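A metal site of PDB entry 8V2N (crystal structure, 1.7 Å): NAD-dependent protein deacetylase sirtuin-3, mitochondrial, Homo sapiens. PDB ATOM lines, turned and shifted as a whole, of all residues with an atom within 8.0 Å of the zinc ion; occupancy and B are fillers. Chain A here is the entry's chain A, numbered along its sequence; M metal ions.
The side-chain sulfur of Cys 163 lies close to the backbone NH of Val 165 (3.2 Å).
The backbone NH (N) of Cys 163 lies within hydrogen-bond range of the backbone carbonyl oxygen (O) of Gly 168.
The backbone NH (N) of Arg 144 lies close to the side-chain sulfur (SG) of Cys 142, at 3.6 Å.
N of Gly 168 sits close to SG of Cys 166 (3.3 Å).
The backbone NH (N) of Val 141 lies close to the side-chain sulfur (SG) of Cys 139.
N of Cys 139 sits at hydrogen-bond distance from O of Arg 144.
Of the 18 residues printed, 4 come within 4 Å of the zinc ion.
SG of Cys 163 binds the zinc ion (2.3 Å).
SG of Cys 142 is bound to the zinc ion (2.3 Å).
SG of Cys 166 binds the zinc ion (2.3 Å).
The zinc ion is bound by SG of Cys 139, at 2.3 Å.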
ATOM      1  N   THR A 138     -19.600   0.580  20.533  1.00  0.00           N
ATOM      2  CA  THR A 138     -19.941   0.904  21.906  1.00  0.00           C
ATOM      3  C   THR A 138     -19.337  -0.164  22.818  1.00  0.00           C
ATOM      4  O   THR A 138     -19.443  -1.338  22.539  1.00  0.00           O
ATOM      5  CB  THR A 138     -21.460   1.016  22.070  1.00  0.00           C
ATOM      6  OG1 THR A 138     -21.898   2.042  21.169  1.00  0.00           O
ATOM      7  CG2 THR A 138     -21.905   1.385  23.477  1.00  0.00           C
ATOM      8  N   CYS A 139     -18.697   0.260  23.908  1.00  0.00           N
ATOM      9  CA  CYS A 139     -18.240  -0.697  24.918  1.00  0.00           C
ATOM     10  C   CYS A 139     -19.446  -1.367  25.582  1.00  0.00           C
ATOM     11  O   CYS A 139     -20.399  -0.690  25.979  1.00  0.00           O
ATOM     12  CB  CYS A 139     -17.415   0.004  25.997  1.00  0.00           C
ATOM     13  SG  CYS A 139     -16.985  -1.173  27.257  1.00  0.00           S
ATOM     14  N   THR A 140     -19.370  -2.696  25.718  1.00  0.00           N
ATOM     15  CA  THR A 140     -20.491  -3.478  26.206  1.00  0.00           C
ATOM     16  C   THR A 140     -20.619  -3.316  27.721  1.00  0.00           C
ATOM     17  O   THR A 140     -21.641  -3.668  28.303  1.00  0.00           O
ATOM     18  CB  THR A 140     -20.330  -4.950  25.848  1.00  0.00           C
ATOM     19  OG1 THR A 140     -19.019  -5.301  26.283  1.00  0.00           O
ATOM     20  CG2 THR A 140     -20.493  -5.206  24.361  1.00  0.00           C
ATOM     21  N   VAL A 141     -19.552  -2.805  28.373  1.00  0.00           N
ATOM     22  CA  VAL A 141     -19.539  -2.693  29.821  1.00  0.00           C
ATOM     23  C   VAL A 141     -19.918  -1.265  30.226  1.00  0.00           C
ATOM     24  O   VAL A 141     -20.949  -1.047  30.835  1.00  0.00           O
ATOM     25  CB  VAL A 141     -18.185  -3.147  30.441  1.00  0.00           C
ATOM     26  CG1 VAL A 141     -18.154  -2.934  31.949  1.00  0.00           C
ATOM     27  CG2 VAL A 141     -17.849  -4.594  30.091  1.00  0.00           C
ATOM     28  N   CYS A 142     -19.078  -0.291  29.832  1.00  0.00           N
ATOM     29  CA  CYS A 142     -19.166   1.063  30.385  1.00  0.00           C
ATOM     30  C   CYS A 142     -19.985   1.984  29.455  1.00  0.00           C
ATOM     31  O   CYS A 142     -20.311   3.106  29.833  1.00  0.00           O
ATOM     32  CB  CYS A 142     -17.778   1.645  30.623  1.00  0.00           C
ATOM     33  SG  CYS A 142     -16.943   2.047  29.153  1.00  0.00           S
ATOM     34  N   GLN A 143     -20.233   1.513  28.211  1.00  0.00           N
ATOM     35  CA  GLN A 143     -21.153   2.183  27.269  1.00  0.00           C
ATOM     36  C   GLN A 143     -20.453   3.362  26.572  1.00  0.00           C
ATOM     37  O   GLN A 143     -21.092   4.141  25.867  1.00  0.00           O
ATOM     38  CB  GLN A 143     -22.464   2.587  27.960  1.00  0.00           C
ATOM     39  CG  GLN A 143     -23.128   1.457  28.745  1.00  0.00           C
ATOM     40  CD  GLN A 143     -23.446   0.252  27.898  1.00  0.00           C
ATOM     41  OE1 GLN A 143     -23.848   0.364  26.744  1.00  0.00           O
ATOM     42  NE2 GLN A 143     -23.255  -0.926  28.477  1.00  0.00           N
ATOM     43  N   ARG A 144     -19.130   3.435  26.713  1.00  0.00           N
ATOM     44  CA  ARG A 144     -18.315   4.419  25.999  1.00  0.00           C
ATOM     45  C   ARG A 144     -18.490   4.237  24.480  1.00  0.00           C
ATOM     46  O   ARG A 144     -18.227   3.167  23.951  1.00  0.00           O
ATOM     47  CB  ARG A 144     -16.840   4.258  26.387  1.00  0.00           C
ATOM     48  CG  ARG A 144     -15.894   5.205  25.654  1.00  0.00           C
ATOM     49  CD  ARG A 144     -14.509   5.190  26.263  1.00  0.00           C
ATOM     50  NE  ARG A 144     -14.501   5.797  27.577  1.00  0.00           N
ATOM     51  CZ  ARG A 144     -14.311   7.094  27.821  1.00  0.00           C
ATOM     52  NH1 ARG A 144     -14.055   7.914  26.816  1.00  0.00           N
ATOM     53  NH2 ARG A 144     -14.352   7.540  29.049  1.00  0.00           N
ATOM     54  N   PRO A 145     -18.893   5.289  23.729  1.00  0.00           N
ATOM     55  CA  PRO A 145     -18.943   5.213  22.267  1.00  0.00           C
ATOM     56  C   PRO A 145     -17.564   5.368  21.640  1.00  0.00           C
ATOM     57  O   PRO A 145     -16.673   5.972  22.229  1.00  0.00           O
ATOM     58  CB  PRO A 145     -19.851   6.398  21.888  1.00  0.00           C
ATOM     59  CG  PRO A 145     -19.626   7.403  23.009  1.00  0.00           C
ATOM     60  CD  PRO A 145     -19.434   6.556  24.254  1.00  0.00           C
ATOM     61  N   PHE A 146     -17.401   4.786  20.461  1.00  0.00           N
ATOM     62  CA  PHE A 146     -16.143   4.810  19.726  1.00  0.00           C
ATOM     63  C   PHE A 146     -16.453   4.980  18.243  1.00  0.00           C
ATOM     64  O   PHE A 146     -17.430   4.435  17.752  1.00  0.00           O
ATOM     65  CB  PHE A 146     -15.401   3.490  19.891  1.00  0.00           C
ATOM     66  CG  PHE A 146     -14.999   3.166  21.309  1.00  0.00           C
ATOM     67  CD1 PHE A 146     -13.847   3.703  21.873  1.00  0.00           C
ATOM     68  CD2 PHE A 146     -15.769   2.310  22.087  1.00  0.00           C
ATOM     69  CE1 PHE A 146     -13.477   3.389  23.163  1.00  0.00           C
ATOM     70  CE2 PHE A 146     -15.393   2.000  23.383  1.00  0.00           C
ATOM     71  CZ  PHE A 146     -14.247   2.544  23.919  1.00  0.00           C
ATOM     72  N   ARG A 162     -11.035  -4.412  22.591  1.00  0.00           N
ATOM     73  CA  ARG A 162     -11.365  -4.249  24.003  1.00  0.00           C
ATOM     74  C   ARG A 162     -11.279  -2.783  24.406  1.00  0.00           C
ATOM     75  O   ARG A 162     -10.411  -2.049  23.941  1.00  0.00           O
ATOM     76  CB  ARG A 162     -10.489  -5.141  24.874  1.00  0.00           C
ATOM     77  CG  ARG A 162     -10.730  -6.634  24.673  1.00  0.00           C
ATOM     78  CD  ARG A 162     -10.938  -7.366  25.964  1.00  0.00           C
ATOM     79  NE  ARG A 162     -11.629  -8.629  25.776  1.00  0.00           N
ATOM     80  CZ  ARG A 162     -11.094  -9.705  25.205  1.00  0.00           C
ATOM     81  NH1 ARG A 162      -9.854  -9.667  24.757  1.00  0.00           N
ATOM     82  NH2 ARG A 162     -11.807 -10.818  25.089  1.00  0.00           N
ATOM     83  N   CYS A 163     -12.149  -2.396  25.339  1.00  0.00           N
ATOM     84  CA  CYS A 163     -12.319  -1.012  25.743  1.00  0.00           C
ATOM     85  C   CYS A 163     -11.097  -0.556  26.531  1.00  0.00           C
ATOM     86  O   CYS A 163     -10.670  -1.255  27.452  1.00  0.00           O
ATOM     87  CB  CYS A 163     -13.551  -0.876  26.604  1.00  0.00           C
ATOM     88  SG  CYS A 163     -13.798   0.720  27.331  1.00  0.00           S
ATOM     89  N   PRO A 164     -10.568   0.639  26.246  1.00  0.00           N
ATOM     90  CA  PRO A 164      -9.476   1.221  27.030  1.00  0.00           C
ATOM     91  C   PRO A 164      -9.816   1.386  28.511  1.00  0.00           C
ATOM     92  O   PRO A 164      -8.944   1.289  29.364  1.00  0.00           O
ATOM     93  CB  PRO A 164      -9.248   2.603  26.384  1.00  0.00           C
ATOM     94  CG  PRO A 164     -10.540   2.877  25.590  1.00  0.00           C
ATOM     95  CD  PRO A 164     -10.994   1.508  25.132  1.00  0.00           C
ATOM     96  N   VAL A 165     -11.101   1.630  28.792  1.00  0.00           N
ATOM     97  CA  VAL A 165     -11.517   2.126  30.093  1.00  0.00           C
ATOM     98  C   VAL A 165     -11.750   0.949  31.040  1.00  0.00           C
ATOM     99  O   VAL A 165     -11.353   0.997  32.197  1.00  0.00           O
ATOM    100  CB  VAL A 165     -12.754   3.034  29.995  1.00  0.00           C
ATOM    101  CG1 VAL A 165     -13.484   3.161  31.340  1.00  0.00           C
ATOM    102  CG2 VAL A 165     -12.373   4.414  29.457  1.00  0.00           C
ATOM    103  N   CYS A 166     -12.382  -0.106  30.531  1.00  0.00           N
ATOM    104  CA  CYS A 166     -12.967  -1.114  31.410  1.00  0.00           C
ATOM    105  C   CYS A 166     -12.635  -2.529  30.907  1.00  0.00           C
ATOM    106  O   CYS A 166     -12.966  -3.509  31.574  1.00  0.00           O
ATOM    107  CB  CYS A 166     -14.477  -0.915  31.545  1.00  0.00           C
ATOM    108  SG  CYS A 166     -15.318  -1.507  30.096  1.00  0.00           S
ATOM    109  N   THR A 167     -11.957  -2.627  29.751  1.00  0.00           N
ATOM    110  CA  THR A 167     -11.513  -3.917  29.215  1.00  0.00           C
ATOM    111  C   THR A 167     -12.688  -4.689  28.596  1.00  0.00           C
ATOM    112  O   THR A 167     -12.501  -5.786  28.067  1.00  0.00           O
ATOM    113  CB  THR A 167     -10.810  -4.770  30.285  1.00  0.00           C
ATOM    114  OG1 THR A 167     -11.787  -5.571  30.978  1.00  0.00           O
ATOM    115  CG2 THR A 167      -9.997  -3.964  31.266  1.00  0.00           C
ATOM    116  N   GLY A 168     -13.898  -4.139  28.697  1.00  0.00           N
ATOM    117  CA  GLY A 168     -15.071  -4.766  28.114  1.00  0.00           C
ATOM    118  C   GLY A 168     -14.947  -4.869  26.584  1.00  0.00           C
ATOM    119  O   GLY A 168     -14.233  -4.096  25.974  1.00  0.00           O
ATOM    120  N   VAL A 169     -15.683  -5.830  25.986  1.00  0.00           N
ATOM    121  CA  VAL A 169     -15.686  -5.977  24.534  1.00  0.00           C
ATOM    122  C   VAL A 169     -16.348  -4.749  23.910  1.00  0.00           C
ATOM    123  O   VAL A 169     -17.416  -4.328  24.329  1.00  0.00           O
ATOM    124  CB  VAL A 169     -16.387  -7.277  24.084  1.00  0.00           C
ATOM    125  CG1 VAL A 169     -16.261  -7.494  22.574  1.00  0.00           C
ATOM    126  CG2 VAL A 169     -15.865  -8.495  24.829  1.00  0.00           C
ATOM    127  N   VAL A 170     -15.695  -4.197  22.891  1.00  0.00           N
ATOM    128  CA  VAL A 170     -16.265  -3.089  22.137  1.00  0.00           C
ATOM    129  C   VAL A 170     -16.995  -3.673  20.924  1.00  0.00           C
ATOM    130  O   VAL A 170     -16.397  -4.348  20.099  1.00  0.00           O
ATOM    131  CB  VAL A 170     -15.193  -2.072  21.713  1.00  0.00           C
ATOM    132  CG1 VAL A 170     -15.768  -0.945  20.845  1.00  0.00           C
ATOM    133  CG2 VAL A 170     -14.469  -1.498  22.907  1.00  0.00           C
HETATM  134 ZN    ZN M   1     -15.646   0.212  28.566  1.00  0.00          ZN
